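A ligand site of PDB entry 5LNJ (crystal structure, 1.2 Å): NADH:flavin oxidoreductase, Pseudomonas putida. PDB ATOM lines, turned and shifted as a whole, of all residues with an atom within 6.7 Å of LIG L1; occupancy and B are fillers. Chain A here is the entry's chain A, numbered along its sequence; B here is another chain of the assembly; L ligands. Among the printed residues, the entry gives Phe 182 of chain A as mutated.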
ATOM      1  N   PRO A  22     -23.251  19.436 -14.267  1.00  0.00           N
ATOM      2  CA  PRO A  22     -23.965  20.695 -14.134  1.00  0.00           C
ATOM      3  C   PRO A  22     -23.967  21.157 -12.681  1.00  0.00           C
ATOM      4  O   PRO A  22     -24.284  20.406 -11.773  1.00  0.00           O
ATOM      5  CB  PRO A  22     -25.380  20.362 -14.667  1.00  0.00           C
ATOM      6  CG  PRO A  22     -25.496  18.848 -14.519  1.00  0.00           C
ATOM      7  CD  PRO A  22     -24.113  18.350 -14.767  1.00  0.00           C
ATOM      8  N   MET A  23     -23.614  22.426 -12.499  1.00  0.00           N
ATOM      9  CA  MET A  23     -23.605  23.047 -11.161  1.00  0.00           C
ATOM     10  C   MET A  23     -24.175  24.465 -11.259  1.00  0.00           C
ATOM     11  O   MET A  23     -23.489  25.413 -11.679  1.00  0.00           O
ATOM     12  CB  MET A  23     -22.204  23.097 -10.536  1.00  0.00           C
ATOM     13  CG  MET A  23     -21.707  21.713 -10.088  1.00  0.00           C
ATOM     14  SD  MET A  23     -20.078  21.767  -9.334  1.00  0.00           S
ATOM     15  CE  MET A  23     -19.087  22.083 -10.760  1.00  0.00           C
ATOM     16  N   CYS A  24     -25.406  24.610 -10.819  1.00  0.00           N
ATOM     17  CA  CYS A  24     -26.057  25.925 -10.720  1.00  0.00           C
ATOM     18  C   CYS A  24     -25.181  26.956 -10.040  1.00  0.00           C
ATOM     19  O   CYS A  24     -24.582  26.690  -8.967  1.00  0.00           O
ATOM     20  CB  CYS A  24     -27.359  25.786  -9.955  1.00  0.00           C
ATOM     21  SG  CYS A  24     -28.733  25.049 -10.873  1.00  0.00           S
ATOM     22  N   TYR A  26     -26.587  30.354  -9.801  1.00  0.00           N
ATOM     23  CA  TYR A  26     -27.542  31.300  -9.216  1.00  0.00           C
ATOM     24  C   TYR A  26     -27.176  32.754  -9.504  1.00  0.00           C
ATOM     25  O   TYR A  26     -27.483  33.631  -8.705  1.00  0.00           O
ATOM     26  CB  TYR A  26     -27.729  31.040  -7.711  1.00  0.00           C
ATOM     27  CG  TYR A  26     -27.981  29.578  -7.368  1.00  0.00           C
ATOM     28  CD1 TYR A  26     -29.275  29.063  -7.378  1.00  0.00           C
ATOM     29  CD2 TYR A  26     -26.926  28.724  -7.072  1.00  0.00           C
ATOM     30  CE1 TYR A  26     -29.509  27.713  -7.079  1.00  0.00           C
ATOM     31  CE2 TYR A  26     -27.150  27.398  -6.788  1.00  0.00           C
ATOM     32  CZ  TYR A  26     -28.447  26.890  -6.774  1.00  0.00           C
ATOM     33  OH  TYR A  26     -28.632  25.564  -6.469  1.00  0.00           O
ATOM     34  N   ALA A  56     -28.052  23.380 -14.813  1.00  0.00           N
ATOM     35  CA  ALA A  56     -29.483  23.272 -15.081  1.00  0.00           C
ATOM     36  C   ALA A  56     -29.996  24.598 -15.664  1.00  0.00           C
ATOM     37  O   ALA A  56     -30.005  25.637 -14.981  1.00  0.00           O
ATOM     38  CB  ALA A  56     -30.226  22.949 -13.791  1.00  0.00           C
ATOM     39  N   ILE A  65     -35.183  26.906 -10.821  1.00  0.00           N
ATOM     40  CA  ILE A  65     -35.225  26.657  -9.383  1.00  0.00           C
ATOM     41  C   ILE A  65     -35.434  27.974  -8.632  1.00  0.00           C
ATOM     42  O   ILE A  65     -36.246  28.031  -7.712  1.00  0.00           O
ATOM     43  CB  ILE A  65     -33.979  25.904  -8.846  1.00  0.00           C
ATOM     44  CG1 ILE A  65     -33.676  24.670  -9.701  1.00  0.00           C
ATOM     45  CG2 ILE A  65     -34.194  25.556  -7.373  1.00  0.00           C
ATOM     46  CD1 ILE A  65     -32.260  24.142  -9.485  1.00  0.00           C
ATOM     47  N   GLN A  98     -27.221  21.031 -19.540  1.00  0.00           N
ATOM     48  CA  GLN A  98     -28.355  20.358 -18.926  1.00  0.00           C
ATOM     49  C   GLN A  98     -29.600  21.232 -19.036  1.00  0.00           C
ATOM     50  O   GLN A  98     -29.586  22.360 -18.527  1.00  0.00           O
ATOM     51  CB  GLN A  98     -28.038  20.053 -17.454  1.00  0.00           C
ATOM     52  CG  GLN A  98     -29.107  19.202 -16.804  1.00  0.00           C
ATOM     53  CD  GLN A  98     -28.918  19.097 -15.321  1.00  0.00           C
ATOM     54  OE1 GLN A  98     -28.937  20.102 -14.634  1.00  0.00           O
ATOM     55  NE2 GLN A  98     -28.773  17.873 -14.801  1.00  0.00           N
ATOM     56  N   PRO A 111     -29.414  29.197  -2.451  1.00  0.00           N
ATOM     57  CA  PRO A 111     -29.066  28.365  -1.306  1.00  0.00           C
ATOM     58  C   PRO A 111     -28.445  29.162  -0.136  1.00  0.00           C
ATOM     59  O   PRO A 111     -28.630  28.750   1.016  1.00  0.00           O
ATOM     60  CB  PRO A 111     -28.093  27.353  -1.903  1.00  0.00           C
ATOM     61  CG  PRO A 111     -28.587  27.201  -3.324  1.00  0.00           C
ATOM     62  CD  PRO A 111     -28.909  28.605  -3.714  1.00  0.00           C
ATOM     63  N   HIS A 177     -32.679  16.887 -17.702  1.00  0.00           N
ATOM     64  CA  HIS A 177     -32.666  16.791 -16.248  1.00  0.00           C
ATOM     65  C   HIS A 177     -33.918  16.112 -15.714  1.00  0.00           C
ATOM     66  O   HIS A 177     -34.920  16.777 -15.390  1.00  0.00           O
ATOM     67  CB  HIS A 177     -32.533  18.181 -15.618  1.00  0.00           C
ATOM     68  CG  HIS A 177     -32.105  18.142 -14.196  1.00  0.00           C
ATOM     69  ND1 HIS A 177     -32.070  16.967 -13.454  1.00  0.00           N
ATOM     70  CD2 HIS A 177     -31.634  19.125 -13.391  1.00  0.00           C
ATOM     71  CE1 HIS A 177     -31.582  17.250 -12.254  1.00  0.00           C
ATOM     72  NE2 HIS A 177     -31.309  18.550 -12.189  1.00  0.00           N
ATOM     73  N   ALA A 179     -33.811  14.275 -12.892  1.00  0.00           N
ATOM     74  CA  ALA A 179     -33.401  13.874 -11.552  1.00  0.00           C
ATOM     75  C   ALA A 179     -33.772  14.899 -10.500  1.00  0.00           C
ATOM     76  O   ALA A 179     -34.400  15.933 -10.782  1.00  0.00           O
ATOM     77  CB  ALA A 179     -31.897  13.548 -11.552  1.00  0.00           C
ATOM     78  N   HIS A 180     -33.397  14.604  -9.252  1.00  0.00           N
ATOM     79  CA  HIS A 180     -33.352  15.564  -8.165  1.00  0.00           C
ATOM     80  C   HIS A 180     -34.712  16.151  -7.775  1.00  0.00           C
ATOM     81  O   HIS A 180     -34.792  17.254  -7.244  1.00  0.00           O
ATOM     82  CB  HIS A 180     -32.281  16.637  -8.444  1.00  0.00           C
ATOM     83  CG  HIS A 180     -30.921  16.034  -8.683  1.00  0.00           C
ATOM     84  ND1 HIS A 180     -29.834  16.735  -9.196  1.00  0.00           N
ATOM     85  CD2 HIS A 180     -30.453  14.776  -8.461  1.00  0.00           C
ATOM     86  CE1 HIS A 180     -28.791  15.935  -9.295  1.00  0.00           C
ATOM     87  NE2 HIS A 180     -29.136  14.745  -8.852  1.00  0.00           N
ATOM     88  N   PHE A 182     -37.161  17.175  -9.460  1.00  0.00           N
ATOM     89  CA  PHE A 182     -37.685  18.198 -10.361  1.00  0.00           C
ATOM     90  C   PHE A 182     -38.774  17.558 -11.235  1.00  0.00           C
ATOM     91  O   PHE A 182     -39.282  16.464 -10.930  1.00  0.00           O
ATOM     92  CB  PHE A 182     -36.506  18.808 -11.122  1.00  0.00           C
ATOM     93  CG  PHE A 182     -35.532  19.541 -10.238  1.00  0.00           C
ATOM     94  CD1 PHE A 182     -35.946  20.416  -9.237  1.00  0.00           C
ATOM     95  CD2 PHE A 182     -34.176  19.340 -10.419  1.00  0.00           C
ATOM     96  CE1 PHE A 182     -35.020  21.106  -8.453  1.00  0.00           C
ATOM     97  CE2 PHE A 182     -33.243  20.027  -9.642  1.00  0.00           C
ATOM     98  CZ  PHE A 182     -33.659  20.912  -8.661  1.00  0.00           C
ATOM     99  N   ARG A 230     -30.030  12.783 -16.920  1.00  0.00           N
ATOM    100  CA  ARG A 230     -29.744  12.530 -15.515  1.00  0.00           C
ATOM    101  C   ARG A 230     -31.023  12.015 -14.888  1.00  0.00           C
ATOM    102  O   ARG A 230     -32.119  12.562 -15.110  1.00  0.00           O
ATOM    103  CB  ARG A 230     -29.269  13.796 -14.782  1.00  0.00           C
ATOM    104  CG  ARG A 230     -28.557  13.450 -13.465  1.00  0.00           C
ATOM    105  CD  ARG A 230     -27.767  14.634 -12.888  1.00  0.00           C
ATOM    106  NE  ARG A 230     -26.647  14.110 -12.103  1.00  0.00           N
ATOM    107  CZ  ARG A 230     -25.752  14.866 -11.463  1.00  0.00           C
ATOM    108  NH1 ARG A 230     -24.705  14.293 -10.887  1.00  0.00           N
ATOM    109  NH2 ARG A 230     -25.884  16.198 -11.410  1.00  0.00           N
ATOM    110  N   PHE A 268     -34.027  12.512  -4.657  1.00  0.00           N
ATOM    111  CA  PHE A 268     -34.413  13.693  -3.872  1.00  0.00           C
ATOM    112  C   PHE A 268     -35.857  14.110  -4.098  1.00  0.00           C
ATOM    113  O   PHE A 268     -36.183  15.289  -4.107  1.00  0.00           O
ATOM    114  CB  PHE A 268     -33.490  14.887  -4.140  1.00  0.00           C
ATOM    115  CG  PHE A 268     -32.032  14.598  -3.926  1.00  0.00           C
ATOM    116  CD1 PHE A 268     -31.480  14.624  -2.658  1.00  0.00           C
ATOM    117  CD2 PHE A 268     -31.202  14.311  -4.994  1.00  0.00           C
ATOM    118  CE1 PHE A 268     -30.127  14.375  -2.460  1.00  0.00           C
ATOM    119  CE2 PHE A 268     -29.848  14.052  -4.805  1.00  0.00           C
ATOM    120  CZ  PHE A 268     -29.314  14.080  -3.540  1.00  0.00           C
ATOM    121  N   TRP A 277     -24.490   9.047   2.413  1.00  0.00           N
ATOM    122  CA  TRP A 277     -23.409   9.799   1.816  1.00  0.00           C
ATOM    123  C   TRP A 277     -22.066   9.232   2.224  1.00  0.00           C
ATOM    124  O   TRP A 277     -21.841   8.881   3.381  1.00  0.00           O
ATOM    125  CB  TRP A 277     -23.457  11.252   2.289  1.00  0.00           C
ATOM    126  CG  TRP A 277     -24.749  11.940   2.023  1.00  0.00           C
ATOM    127  CD1 TRP A 277     -25.713  12.280   2.925  1.00  0.00           C
ATOM    128  CD2 TRP A 277     -25.230  12.375   0.745  1.00  0.00           C
ATOM    129  NE1 TRP A 277     -26.757  12.903   2.287  1.00  0.00           N
ATOM    130  CE2 TRP A 277     -26.484  12.974   0.943  1.00  0.00           C
ATOM    131  CE3 TRP A 277     -24.720  12.309  -0.546  1.00  0.00           C
ATOM    132  CZ2 TRP A 277     -27.226  13.508  -0.090  1.00  0.00           C
ATOM    133  CZ3 TRP A 277     -25.457  12.827  -1.583  1.00  0.00           C
ATOM    134  CH2 TRP A 277     -26.686  13.432  -1.350  1.00  0.00           C
ATOM    135  N   TRP A 301     -21.207  12.635  -6.575  1.00  0.00           N
ATOM    136  CA  TRP A 301     -21.490  12.538  -5.143  1.00  0.00           C
ATOM    137  C   TRP A 301     -20.425  11.794  -4.376  1.00  0.00           C
ATOM    138  O   TRP A 301     -20.726  10.856  -3.622  1.00  0.00           O
ATOM    139  CB  TRP A 301     -22.848  11.917  -4.880  1.00  0.00           C
ATOM    140  CG  TRP A 301     -23.963  12.557  -5.621  1.00  0.00           C
ATOM    141  CD1 TRP A 301     -24.621  12.043  -6.700  1.00  0.00           C
ATOM    142  CD2 TRP A 301     -24.591  13.805  -5.328  1.00  0.00           C
ATOM    143  NE1 TRP A 301     -25.593  12.912  -7.111  1.00  0.00           N
ATOM    144  CE2 TRP A 301     -25.596  13.999  -6.282  1.00  0.00           C
ATOM    145  CE3 TRP A 301     -24.377  14.794  -4.367  1.00  0.00           C
ATOM    146  CZ2 TRP A 301     -26.392  15.143  -6.308  1.00  0.00           C
ATOM    147  CZ3 TRP A 301     -25.171  15.920  -4.383  1.00  0.00           C
ATOM    148  CH2 TRP A 301     -26.166  16.080  -5.343  1.00  0.00           C
ATOM    149  N   ARG A 325     -17.734  19.596  -6.821  1.00  0.00           N
ATOM    150  CA  ARG A 325     -17.234  20.552  -5.833  1.00  0.00           C
ATOM    151  C   ARG A 325     -15.731  20.723  -5.884  1.00  0.00           C
ATOM    152  O   ARG A 325     -15.241  21.835  -5.665  1.00  0.00           O
ATOM    153  CB  ARG A 325     -17.705  20.176  -4.435  1.00  0.00           C
ATOM    154  CG  ARG A 325     -19.170  20.544  -4.240  1.00  0.00           C
ATOM    155  CD  ARG A 325     -19.762  19.939  -3.006  1.00  0.00           C
ATOM    156  NE  ARG A 325     -19.890  18.510  -3.194  1.00  0.00           N
ATOM    157  CZ  ARG A 325     -20.402  17.690  -2.286  1.00  0.00           C
ATOM    158  NH1 ARG A 325     -20.794  18.166  -1.111  1.00  0.00           N
ATOM    159  NH2 ARG A 325     -20.484  16.384  -2.540  1.00  0.00           N
ATOM    160  N   TRP B 357     -20.840  26.161  -0.948  1.00  0.00           N
ATOM    161  CA  TRP B 357     -20.742  24.694  -1.106  1.00  0.00           C
ATOM    162  C   TRP B 357     -19.501  24.109  -0.499  1.00  0.00           C
ATOM    163  O   TRP B 357     -19.415  22.902  -0.317  1.00  0.00           O
ATOM    164  CB  TRP B 357     -20.810  24.359  -2.592  1.00  0.00           C
ATOM    165  CG  TRP B 357     -22.002  24.991  -3.216  1.00  0.00           C
ATOM    166  CD1 TRP B 357     -21.995  26.085  -4.014  1.00  0.00           C
ATOM    167  CD2 TRP B 357     -23.364  24.653  -2.974  1.00  0.00           C
ATOM    168  NE1 TRP B 357     -23.286  26.434  -4.325  1.00  0.00           N
ATOM    169  CE2 TRP B 357     -24.145  25.562  -3.725  1.00  0.00           C
ATOM    170  CE3 TRP B 357     -24.003  23.664  -2.231  1.00  0.00           C
ATOM    171  CZ2 TRP B 357     -25.521  25.502  -3.744  1.00  0.00           C
ATOM    172  CZ3 TRP B 357     -25.371  23.614  -2.260  1.00  0.00           C
ATOM    173  CH2 TRP B 357     -26.126  24.521  -3.030  1.00  0.00           C
HETATM  174  O1  LIG L   1     -30.099  19.484  -9.733  1.00  0.00           O
HETATM  175  C1  LIG L   1     -29.730  20.300  -8.942  1.00  0.00           C
HETATM  176  C2  LIG L   1     -29.757  21.692  -8.885  1.00  0.00           C
HETATM  177  C3  LIG L   1     -29.194  22.391  -7.830  1.00  0.00           C
HETATM  178  C4  LIG L   1     -28.548  21.676  -6.827  1.00  0.00           C
HETATM  179  O2  LIG L   1     -29.128  19.609  -7.904  1.00  0.00           O
HETATM  180  C5  LIG L   1     -28.530  20.284  -6.863  1.00  0.00           C
HETATM  181  C6  LIG L   1     -27.901  19.497  -5.917  1.00  0.00           C
HETATM  182  C7  LIG L   1     -27.293  20.093  -4.835  1.00  0.00           C
HETATM  183  O3  LIG L   1     -26.674  19.359  -3.863  1.00  0.00           O
HETATM  184  C8  LIG L   1     -27.295  21.481  -4.752  1.00  0.00           C
HETATM  185  C9  LIG L   1     -27.915  22.259  -5.728  1.00  0.00           C
HETATM  186  C1  LG2 L   2     -25.094  20.876  -8.018  1.00  0.00           C
HETATM  187  N1  LG2 L   2     -25.688  19.693  -8.567  1.00  0.00           N
HETATM  188  C2  LG2 L   2     -26.532  19.841  -9.682  1.00  0.00           C
HETATM  189  N2  LG2 L   2     -26.977  18.718 -10.287  1.00  0.00           N
HETATM  190  C3  LG2 L   2     -27.664  18.825 -11.466  1.00  0.00           C
HETATM  191  O1  LG2 L   2     -28.118  17.789 -12.029  1.00  0.00           O
HETATM  192  N3  LG2 L   2     -27.929  20.081 -11.985  1.00  0.00           N
HETATM  193  C4  LG2 L   2     -27.393  21.228 -11.461  1.00  0.00           C
HETATM  194  O2  LG2 L   2     -27.460  22.305 -12.092  1.00  0.00           O
HETATM  195  C5  LG2 L   2     -26.861  21.119 -10.155  1.00  0.00           C
HETATM  196  N4  LG2 L   2     -26.490  22.282  -9.421  1.00  0.00           N
HETATM  197  C6  LG2 L   2     -25.495  22.142  -8.440  1.00  0.00           C
HETATM  198  C7  LG2 L   2     -24.834  23.296  -7.930  1.00  0.00           C
HETATM  199  C8  LG2 L   2     -23.741  23.155  -7.058  1.00  0.00           C
HETATM  200  C9  LG2 L   2     -23.003  24.384  -6.693  1.00  0.00           C
HETATM  201  C10 LG2 L   2     -23.422  21.887  -6.554  1.00  0.00           C
HETATM  202  C11 LG2 L   2     -22.273  21.724  -5.604  1.00  0.00           C
HETATM  203  C12 LG2 L   2     -24.122  20.761  -6.983  1.00  0.00           C
HETATM  204  C13 LG2 L   2     -25.118  18.347  -8.268  1.00  0.00           C
HETATM  205  C14 LG2 L   2     -23.743  18.160  -8.914  1.00  0.00           C
HETATM  206  O3  LG2 L   2     -23.857  17.990 -10.339  1.00  0.00           O
HETATM  207  C15 LG2 L   2     -23.025  16.927  -8.347  1.00  0.00           C
HETATM  208  O4  LG2 L   2     -23.856  15.769  -8.512  1.00  0.00           O
HETATM  209  C16 LG2 L   2     -22.670  17.064  -6.866  1.00  0.00           C
HETATM  210  O5  LG2 L   2     -21.895  18.255  -6.696  1.00  0.00           O
HETATM  211  C17 LG2 L   2     -21.928  15.829  -6.347  1.00  0.00           C
HETATM  212  O6  LG2 L   2     -20.632  15.680  -6.953  1.00  0.00           O
HETATM  213  P1  LG2 L   2     -19.286  16.121  -6.126  1.00  0.00           P
HETATM  214  O7  LG2 L   2     -19.480  17.580  -5.810  1.00  0.00           O
HETATM  215  O8  LG2 L   2     -19.253  15.282  -4.876  1.00  0.00           O
HETATM  216  O9  LG2 L   2     -18.153  15.875  -7.079  1.00  0.00           O
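ND1 of His 180 lies within hydrogen-bond range of O1 of LIG L1, at 2.8 Å.
NE2 of His 177 sits at hydrogen-bond distance from O1 of LIG L1, at 2.9 Å.
A ring nitrogen (ND1) of His 180 lies close to an oxygen (O1) of LG2 L2, at 3.5 Å.
An oxygen (O1) of LG2 L2 sits at hydrogen-bond distance from a ring nitrogen (NE2) of His 177.
O6 of LG2 L2 sits at hydrogen-bond distance from N of Trp 301.
N of Cys 24 sits close to O2 of LG2 L2, 3.3 Å away.
An oxygen (O2) of LG2 L2 is in hydrogen-bond range of the side-chain sulfur (SG) of Cys 24, 3.3 Å away.
OE1 of Gln 98 is in hydrogen-bond range of N3 of LG2 L2 (2.8 Å).
N of Ala 56 is in hydrogen-bond range of O2 of LG2 L2, 3.0 Å away.
The guanidinium group (NH2) of Arg 230 is in hydrogen-bond range of an oxygen (O1) of LG2 L2 (2.8 Å).
O of Pro 22 is in hydrogen-bond range of O3 of LG2 L2.
An oxygen (O7) of LG2 L2 sits at hydrogen-bond distance from the backbone NH of Arg 325 (2.9 Å).
NE of Arg 325 lies within salt-bridge range of O7 of LG2 L2 (2.8 Å).
An oxygen (O1) of LIG L1 sits close to a nitrogen (N3) of LG2 L2.
A ring nitrogen (ND1) of His 177 is in hydrogen-bond range of the backbone NH (N) of Ala 179, at 3.3 Å.
Residues that only touch LIG L1: Phe 182 (3.2 Å), Tyr 26 (3.5 Å), Ile 65 (3.6 Å), Trp 301 (3.6 Å) and Trp 357 of chain B (3.7 Å).
Hydrophobic or aromatic side chains within 4 Å of LIG L1: Ile 65, His 177, His 180, Phe 182, Trp 301 and Trp 357 of chain B.
Seven residues have an atom within 4 Å of LIG L1: Tyr 26, Ile 65, His 177, His 180, Phe 182, Trp 301 and Trp 357 of chain B.
The nearest printed residue that does not touch LIG L1 is Cys 24 (4.03 Å).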
